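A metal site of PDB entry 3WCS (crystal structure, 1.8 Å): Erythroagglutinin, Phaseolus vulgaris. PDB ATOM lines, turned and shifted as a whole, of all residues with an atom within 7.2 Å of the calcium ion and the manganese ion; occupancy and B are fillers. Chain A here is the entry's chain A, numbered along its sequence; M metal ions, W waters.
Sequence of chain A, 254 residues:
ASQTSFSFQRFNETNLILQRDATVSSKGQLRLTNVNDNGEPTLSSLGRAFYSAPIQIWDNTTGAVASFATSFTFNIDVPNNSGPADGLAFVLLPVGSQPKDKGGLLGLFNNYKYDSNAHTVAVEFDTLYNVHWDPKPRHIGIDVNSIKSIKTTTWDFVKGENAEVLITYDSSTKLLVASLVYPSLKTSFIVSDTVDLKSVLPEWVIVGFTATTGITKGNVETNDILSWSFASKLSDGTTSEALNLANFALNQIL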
ATOM      1  N   ASP A  86       0.052 -23.227 -17.599  1.00  0.00           N
ATOM      2  CA  ASP A  86       1.479 -23.396 -17.987  1.00  0.00           C
ATOM      3  C   ASP A  86       1.694 -24.681 -18.764  1.00  0.00           C
ATOM      4  O   ASP A  86       2.728 -24.856 -19.447  1.00  0.00           O
ATOM      5  CB  ASP A  86       2.341 -23.460 -16.723  1.00  0.00           C
ATOM      6  CG  ASP A  86       2.869 -22.122 -16.322  1.00  0.00           C
ATOM      7  OD1 ASP A  86       3.850 -21.663 -16.973  1.00  0.00           O
ATOM      8  OD2 ASP A  86       2.357 -21.540 -15.334  1.00  0.00           O
ATOM      9  N   GLY A  87       0.762 -25.629 -18.615  1.00  0.00           N
ATOM     10  CA  GLY A  87       0.803 -26.856 -19.394  1.00  0.00           C
ATOM     11  C   GLY A  87       0.506 -28.068 -18.544  1.00  0.00           C
ATOM     12  O   GLY A  87       0.141 -27.938 -17.368  1.00  0.00           O
ATOM     13  N   GLY A 103       3.349 -23.261 -11.350  1.00  0.00           N
ATOM     14  CA  GLY A 103       3.664 -22.471 -12.553  1.00  0.00           C
ATOM     15  C   GLY A 103       4.498 -23.229 -13.588  1.00  0.00           C
ATOM     16  O   GLY A 103       4.224 -24.376 -13.917  1.00  0.00           O
ATOM     17  N   GLY A 104       5.561 -22.573 -14.079  1.00  0.00           N
ATOM     18  CA  GLY A 104       6.361 -23.162 -15.142  1.00  0.00           C
ATOM     19  C   GLY A 104       7.143 -24.418 -14.740  1.00  0.00           C
ATOM     20  O   GLY A 104       7.678 -25.108 -15.574  1.00  0.00           O
ATOM     21  N   LEU A 105       7.224 -24.692 -13.455  1.00  0.00           N
ATOM     22  CA  LEU A 105       7.911 -25.893 -13.004  1.00  0.00           C
ATOM     23  C   LEU A 105       6.970 -27.116 -12.952  1.00  0.00           C
ATOM     24  O   LEU A 105       7.406 -28.239 -12.647  1.00  0.00           O
ATOM     25  CB  LEU A 105       8.575 -25.623 -11.652  1.00  0.00           C
ATOM     26  CG  LEU A 105       9.668 -24.528 -11.725  1.00  0.00           C
ATOM     27  CD1 LEU A 105      10.173 -24.137 -10.338  1.00  0.00           C
ATOM     28  CD2 LEU A 105      10.805 -24.928 -12.657  1.00  0.00           C
ATOM     29  N   LEU A 106       5.701 -26.886 -13.272  1.00  0.00           N
ATOM     30  CA  LEU A 106       4.740 -27.984 -13.547  1.00  0.00           C
ATOM     31  C   LEU A 106       4.449 -28.937 -12.372  1.00  0.00           C
ATOM     32  O   LEU A 106       3.913 -30.041 -12.558  1.00  0.00           O
ATOM     33  CB  LEU A 106       5.164 -28.766 -14.802  1.00  0.00           C
ATOM     34  CG  LEU A 106       5.238 -27.993 -16.122  1.00  0.00           C
ATOM     35  CD1 LEU A 106       5.633 -28.877 -17.286  1.00  0.00           C
ATOM     36  CD2 LEU A 106       3.943 -27.258 -16.441  1.00  0.00           C
ATOM     37  N   GLU A 124       6.100 -33.463 -21.464  1.00  0.00           N
ATOM     38  CA  GLU A 124       5.400 -32.210 -21.203  1.00  0.00           C
ATOM     39  C   GLU A 124       4.767 -31.602 -22.438  1.00  0.00           C
ATOM     40  O   GLU A 124       5.269 -31.764 -23.556  1.00  0.00           O
ATOM     41  CB  GLU A 124       6.318 -31.173 -20.548  1.00  0.00           C
ATOM     42  CG  GLU A 124       7.511 -30.726 -21.428  1.00  0.00           C
ATOM     43  CD  GLU A 124       8.191 -29.450 -20.913  1.00  0.00           C
ATOM     44  OE1 GLU A 124       8.574 -29.464 -19.711  1.00  0.00           O
ATOM     45  OE2 GLU A 124       8.351 -28.426 -21.659  1.00  0.00           O
ATOM     46  N   PHE A 125       3.602 -30.966 -22.222  1.00  0.00           N
ATOM     47  CA  PHE A 125       2.860 -30.251 -23.244  1.00  0.00           C
ATOM     48  C   PHE A 125       2.811 -28.839 -22.710  1.00  0.00           C
ATOM     49  O   PHE A 125       2.004 -28.513 -21.848  1.00  0.00           O
ATOM     50  CB  PHE A 125       1.474 -30.939 -23.414  1.00  0.00           C
ATOM     51  CG  PHE A 125       1.624 -32.344 -23.882  1.00  0.00           C
ATOM     52  CD1 PHE A 125       1.642 -32.644 -25.241  1.00  0.00           C
ATOM     53  CD2 PHE A 125       1.862 -33.379 -22.965  1.00  0.00           C
ATOM     54  CE1 PHE A 125       1.855 -33.926 -25.691  1.00  0.00           C
ATOM     55  CE2 PHE A 125       2.088 -34.669 -23.413  1.00  0.00           C
ATOM     56  CZ  PHE A 125       2.073 -34.948 -24.757  1.00  0.00           C
ATOM     57  N   ASP A 126       3.784 -28.041 -23.158  1.00  0.00           N
ATOM     58  CA  ASP A 126       4.169 -26.759 -22.491  1.00  0.00           C
ATOM     59  C   ASP A 126       3.605 -25.597 -23.318  1.00  0.00           C
ATOM     60  O   ASP A 126       3.950 -25.430 -24.491  1.00  0.00           O
ATOM     61  CB  ASP A 126       5.724 -26.705 -22.395  1.00  0.00           C
ATOM     62  CG  ASP A 126       6.270 -25.538 -21.538  1.00  0.00           C
ATOM     63  OD1 ASP A 126       5.477 -24.619 -21.255  1.00  0.00           O
ATOM     64  OD2 ASP A 126       7.505 -25.553 -21.135  1.00  0.00           O
ATOM     65  N   THR A 127       2.724 -24.808 -22.687  1.00  0.00           N
ATOM     66  CA  THR A 127       1.994 -23.751 -23.378  1.00  0.00           C
ATOM     67  C   THR A 127       2.497 -22.364 -23.084  1.00  0.00           C
ATOM     68  O   THR A 127       1.912 -21.379 -23.580  1.00  0.00           O
ATOM     69  CB  THR A 127       0.501 -23.780 -22.975  1.00  0.00           C
ATOM     70  OG1 THR A 127       0.385 -23.585 -21.573  1.00  0.00           O
ATOM     71  CG2 THR A 127      -0.124 -25.114 -23.392  1.00  0.00           C
ATOM     72  N   LEU A 128       3.549 -22.261 -22.270  1.00  0.00           N
ATOM     73  CA  LEU A 128       4.068 -20.955 -21.832  1.00  0.00           C
ATOM     74  C   LEU A 128       5.593 -20.934 -21.906  1.00  0.00           C
ATOM     75  O   LEU A 128       6.279 -21.727 -21.272  1.00  0.00           O
ATOM     76  CB  LEU A 128       3.604 -20.622 -20.409  1.00  0.00           C
ATOM     77  CG  LEU A 128       4.052 -19.154 -20.180  1.00  0.00           C
ATOM     78  CD1 LEU A 128       2.947 -18.119 -20.000  1.00  0.00           C
ATOM     79  CD2 LEU A 128       5.263 -19.029 -19.245  1.00  0.00           C
ATOM     80  N   TYR A 129       6.098 -19.975 -22.683  1.00  0.00           N
ATOM     81  CA  TYR A 129       7.563 -19.787 -22.825  1.00  0.00           C
ATOM     82  C   TYR A 129       8.195 -19.226 -21.555  1.00  0.00           C
ATOM     83  O   TYR A 129       7.905 -18.084 -21.158  1.00  0.00           O
ATOM     84  CB  TYR A 129       7.785 -18.850 -23.998  1.00  0.00           C
ATOM     85  CG  TYR A 129       9.171 -18.212 -24.080  1.00  0.00           C
ATOM     86  CD1 TYR A 129      10.298 -18.991 -24.166  1.00  0.00           C
ATOM     87  CD2 TYR A 129       9.311 -16.835 -24.027  1.00  0.00           C
ATOM     88  CE1 TYR A 129      11.565 -18.384 -24.257  1.00  0.00           C
ATOM     89  CE2 TYR A 129      10.557 -16.219 -24.110  1.00  0.00           C
ATOM     90  CZ  TYR A 129      11.671 -16.998 -24.216  1.00  0.00           C
ATOM     91  OH  TYR A 129      12.915 -16.369 -24.294  1.00  0.00           O
ATOM     92  N   ASN A 130       9.065 -20.020 -20.925  1.00  0.00           N
ATOM     93  CA  ASN A 130       9.736 -19.603 -19.704  1.00  0.00           C
ATOM     94  C   ASN A 130      11.146 -19.240 -20.138  1.00  0.00           C
ATOM     95  O   ASN A 130      11.918 -20.094 -20.546  1.00  0.00           O
ATOM     96  CB  ASN A 130       9.741 -20.730 -18.663  1.00  0.00           C
ATOM     97  CG  ASN A 130       8.377 -20.925 -18.011  1.00  0.00           C
ATOM     98  OD1 ASN A 130       7.640 -21.879 -18.334  1.00  0.00           O
ATOM     99  ND2 ASN A 130       8.046 -20.023 -17.078  1.00  0.00           N
ATOM    100  N   VAL A 131      11.444 -17.947 -20.082  1.00  0.00           N
ATOM    101  CA  VAL A 131      12.673 -17.397 -20.682  1.00  0.00           C
ATOM    102  C   VAL A 131      13.980 -18.076 -20.289  1.00  0.00           C
ATOM    103  O   VAL A 131      14.926 -18.143 -21.089  1.00  0.00           O
ATOM    104  CB  VAL A 131      12.736 -15.861 -20.419  1.00  0.00           C
ATOM    105  CG1 VAL A 131      12.830 -15.557 -18.929  1.00  0.00           C
ATOM    106  CG2 VAL A 131      13.883 -15.221 -21.183  1.00  0.00           C
ATOM    107  N   TRP A 133      14.667 -21.236 -19.636  1.00  0.00           N
ATOM    108  CA  TRP A 133      14.897 -22.615 -20.089  1.00  0.00           C
ATOM    109  C   TRP A 133      14.190 -23.123 -21.321  1.00  0.00           C
ATOM    110  O   TRP A 133      14.640 -24.070 -21.926  1.00  0.00           O
ATOM    111  CB  TRP A 133      14.691 -23.598 -18.930  1.00  0.00           C
ATOM    112  CG  TRP A 133      13.245 -23.691 -18.492  1.00  0.00           C
ATOM    113  CD1 TRP A 133      12.238 -24.443 -19.079  1.00  0.00           C
ATOM    114  CD2 TRP A 133      12.637 -23.059 -17.331  1.00  0.00           C
ATOM    115  NE1 TRP A 133      11.043 -24.281 -18.389  1.00  0.00           N
ATOM    116  CE2 TRP A 133      11.223 -23.479 -17.321  1.00  0.00           C
ATOM    117  CE3 TRP A 133      13.082 -22.190 -16.334  1.00  0.00           C
ATOM    118  CZ2 TRP A 133      10.343 -23.050 -16.357  1.00  0.00           C
ATOM    119  CZ3 TRP A 133      12.182 -21.764 -15.367  1.00  0.00           C
ATOM    120  CH2 TRP A 133      10.835 -22.181 -15.386  1.00  0.00           C
ATOM    121  N   ASP A 134      13.047 -22.537 -21.686  1.00  0.00           N
ATOM    122  CA  ASP A 134      12.236 -23.052 -22.798  1.00  0.00           C
ATOM    123  C   ASP A 134      12.639 -22.516 -24.181  1.00  0.00           C
ATOM    124  O   ASP A 134      13.074 -21.377 -24.277  1.00  0.00           O
ATOM    125  CB  ASP A 134      10.761 -22.651 -22.596  1.00  0.00           C
ATOM    126  CG  ASP A 134       9.993 -23.605 -21.658  1.00  0.00           C
ATOM    127  OD1 ASP A 134      10.234 -24.858 -21.631  1.00  0.00           O
ATOM    128  OD2 ASP A 134       9.066 -23.058 -20.994  1.00  0.00           O
ATOM    129  N   PRO A 135      12.406 -23.313 -25.259  1.00  0.00           N
ATOM    130  CA  PRO A 135      12.339 -22.764 -26.611  1.00  0.00           C
ATOM    131  C   PRO A 135      11.122 -21.839 -26.681  1.00  0.00           C
ATOM    132  O   PRO A 135      10.161 -22.030 -25.931  1.00  0.00           O
ATOM    133  CB  PRO A 135      12.148 -23.995 -27.501  1.00  0.00           C
ATOM    134  CG  PRO A 135      11.551 -25.040 -26.613  1.00  0.00           C
ATOM    135  CD  PRO A 135      11.993 -24.746 -25.211  1.00  0.00           C
ATOM    136  N   PRO A 137       8.729 -21.250 -29.161  1.00  0.00           N
ATOM    137  CA  PRO A 137       7.444 -21.838 -29.569  1.00  0.00           C
ATOM    138  C   PRO A 137       6.932 -22.821 -28.528  1.00  0.00           C
ATOM    139  O   PRO A 137       7.725 -23.503 -27.875  1.00  0.00           O
ATOM    140  CB  PRO A 137       7.764 -22.584 -30.865  1.00  0.00           C
ATOM    141  CG  PRO A 137       9.086 -21.995 -31.347  1.00  0.00           C
ATOM    142  CD  PRO A 137       9.817 -21.658 -30.085  1.00  0.00           C
ATOM    143  N   HIS A 139       5.539 -26.293 -27.203  1.00  0.00           N
ATOM    144  CA  HIS A 139       6.333 -27.478 -27.512  1.00  0.00           C
ATOM    145  C   HIS A 139       5.903 -28.697 -26.736  1.00  0.00           C
ATOM    146  O   HIS A 139       5.303 -28.594 -25.650  1.00  0.00           O
ATOM    147  CB  HIS A 139       7.842 -27.188 -27.253  1.00  0.00           C
ATOM    148  CG  HIS A 139       8.157 -26.654 -25.870  1.00  0.00           C
ATOM    149  ND1 HIS A 139       8.023 -25.351 -25.545  1.00  0.00           N
ATOM    150  CD2 HIS A 139       8.555 -27.323 -24.699  1.00  0.00           C
ATOM    151  CE1 HIS A 139       8.368 -25.178 -24.246  1.00  0.00           C
ATOM    152  NE2 HIS A 139       8.682 -26.397 -23.703  1.00  0.00           N
ATOM    153  N   ILE A 140       6.212 -29.860 -27.301  1.00  0.00           N
ATOM    154  CA  ILE A 140       6.155 -31.109 -26.540  1.00  0.00           C
ATOM    155  C   ILE A 140       7.601 -31.365 -26.169  1.00  0.00           C
ATOM    156  O   ILE A 140       8.486 -31.171 -27.001  1.00  0.00           O
ATOM    157  CB  ILE A 140       5.629 -32.269 -27.392  1.00  0.00           C
ATOM    158  CG1 ILE A 140       4.263 -31.915 -27.999  1.00  0.00           C
ATOM    159  CG2 ILE A 140       5.597 -33.575 -26.597  1.00  0.00           C
ATOM    160  CD1 ILE A 140       3.922 -32.785 -29.189  1.00  0.00           C
ATOM    161  N   GLY A 141       7.842 -31.701 -24.912  1.00  0.00           N
ATOM    162  CA  GLY A 141       9.229 -31.959 -24.459  1.00  0.00           C
ATOM    163  C   GLY A 141       9.348 -33.253 -23.670  1.00  0.00           C
ATOM    164  O   GLY A 141       8.415 -33.649 -22.975  1.00  0.00           O
ATOM    165  N   ASP A 143      11.288 -34.730 -20.590  1.00  0.00           N
ATOM    166  CA  ASP A 143      11.937 -34.202 -19.384  1.00  0.00           C
ATOM    167  C   ASP A 143      12.513 -35.338 -18.580  1.00  0.00           C
ATOM    168  O   ASP A 143      11.781 -36.258 -18.163  1.00  0.00           O
ATOM    169  CB  ASP A 143      10.937 -33.442 -18.490  1.00  0.00           C
ATOM    170  CG  ASP A 143      10.396 -32.185 -19.130  1.00  0.00           C
ATOM    171  OD1 ASP A 143      10.835 -31.862 -20.248  1.00  0.00           O
ATOM    172  OD2 ASP A 143       9.506 -31.538 -18.513  1.00  0.00           O
ATOM    173  N   ILE A 147      13.373 -29.508 -15.654  1.00  0.00           N
ATOM    174  CA  ILE A 147      12.374 -28.785 -16.462  1.00  0.00           C
ATOM    175  C   ILE A 147      12.966 -28.371 -17.818  1.00  0.00           C
ATOM    176  O   ILE A 147      12.233 -28.050 -18.755  1.00  0.00           O
ATOM    177  CB  ILE A 147      11.759 -27.581 -15.706  1.00  0.00           C
ATOM    178  CG1 ILE A 147      10.427 -27.139 -16.332  1.00  0.00           C
ATOM    179  CG2 ILE A 147      12.719 -26.384 -15.725  1.00  0.00           C
ATOM    180  CD1 ILE A 147       9.281 -28.140 -16.165  1.00  0.00           C
ATOM    181  N   LYS A 148      14.311 -28.358 -17.940  1.00  0.00           N
ATOM    182  CA  LYS A 148      14.939 -28.096 -19.231  1.00  0.00           C
ATOM    183  C   LYS A 148      14.944 -29.378 -20.038  1.00  0.00           C
ATOM    184  O   LYS A 148      15.800 -30.264 -19.804  1.00  0.00           O
ATOM    185  CB  LYS A 148      16.393 -27.569 -19.062  1.00  0.00           C
ATOM    186  CG  LYS A 148      17.023 -27.164 -20.383  1.00  0.00           C
ATOM    187  CD  LYS A 148      18.548 -27.051 -20.289  1.00  0.00           C
ATOM    188  CE  LYS A 148      19.135 -27.120 -21.684  1.00  0.00           C
ATOM    189  NZ  LYS A 148      20.618 -27.342 -21.702  1.00  0.00           N
ATOM    190  N   SER A 149      14.025 -29.490 -21.001  1.00  0.00           N
ATOM    191  CA  SER A 149      13.777 -30.769 -21.712  1.00  0.00           C
ATOM    192  C   SER A 149      15.024 -31.244 -22.411  1.00  0.00           C
ATOM    193  O   SER A 149      15.740 -30.421 -22.971  1.00  0.00           O
ATOM    194  CB  SER A 149      12.675 -30.601 -22.751  1.00  0.00           C
ATOM    195  OG  SER A 149      11.492 -30.138 -22.117  1.00  0.00           O
ATOM    196  N   THR A 152      12.897 -31.379 -27.583  1.00  0.00           N
ATOM    197  CA  THR A 152      11.558 -30.805 -27.840  1.00  0.00           C
ATOM    198  C   THR A 152      11.211 -30.833 -29.322  1.00  0.00           C
ATOM    199  O   THR A 152      12.088 -30.962 -30.177  1.00  0.00           O
ATOM    200  CB  THR A 152      11.435 -29.345 -27.332  1.00  0.00           C
ATOM    201  OG1 THR A 152      12.399 -28.510 -28.004  1.00  0.00           O
ATOM    202  CG2 THR A 152      11.622 -29.246 -25.803  1.00  0.00           C
HETATM  203 CA    CA M   1       7.058 -23.499 -19.932  1.00  0.00          CA
HETATM  204 MN    MN M   2       9.168 -26.567 -21.739  1.00  0.00          MN
HETATM  205  O   HOH W   1       8.050 -25.066 -18.512  1.00  0.00           O
HETATM  206  O   HOH W   2       5.065 -23.586 -18.775  1.00  0.00           O
HETATM  207  O   HOH W   3       9.541 -26.999 -19.860  1.00  0.00           O
HETATM  208  O   HOH W   4      10.981 -27.267 -22.209  1.00  0.00           O
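OD1 of Asp 134 sits close to NE1 of Trp 133 (3.4 Å).
A ring nitrogen (ND1) of His 139 is in hydrogen-bond range of the backbone carbonyl oxygen of Pro 137 (3.0 Å).
The side-chain carboxylate (OD2) of Asp 143 sits close to the side-chain carboxylate (OE1) of Glu 124, 2.6 Å away.
The backbone carbonyl oxygen of Gly 141 is in hydrogen-bond range of the backbone NH of Glu 124, at 2.8 Å.
The nearest printed residue that does not touch the calcium ion is Trp 133 (4.3 Å).
The calcium ion is bound by water W2 (2.3 Å), the side-chain carboxylate (OD2) of Asp 134 (2.3 Å), water W1 (2.3 Å), the side-chain carboxylate (OD1) of Asp 126 (2.3 Å), the side-chain amide oxygen (OD1) of Asn 130 (2.3 Å), the backbone carbonyl oxygen (O) of Leu 128 (2.4 Å) and the side-chain carboxylate (OD2) of Asp 126 (2.4 Å).
The calcium ion has seven donor atoms within binding distance.
Water W1 lies within hydrogen-bond range of the backbone carbonyl oxygen (O) of Gly 104 and the indole nitrogen (NE1) of Trp 133.
Water W3 lies within hydrogen-bond range of OE1 of Glu 124, O of Ile 147 and NE1 of Trp 133.
The nearest printed residue that does not touch the manganese ion is Ser 149 (4.3 Å).
The manganese ion is bound by water W3, water W4, the side-chain carboxylate of Asp 134, a ring nitrogen (NE2) of His 139, the side-chain carboxylate of Glu 124 and the side-chain carboxylate of Asp 126.
The manganese ion has six donor atoms within binding distance.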
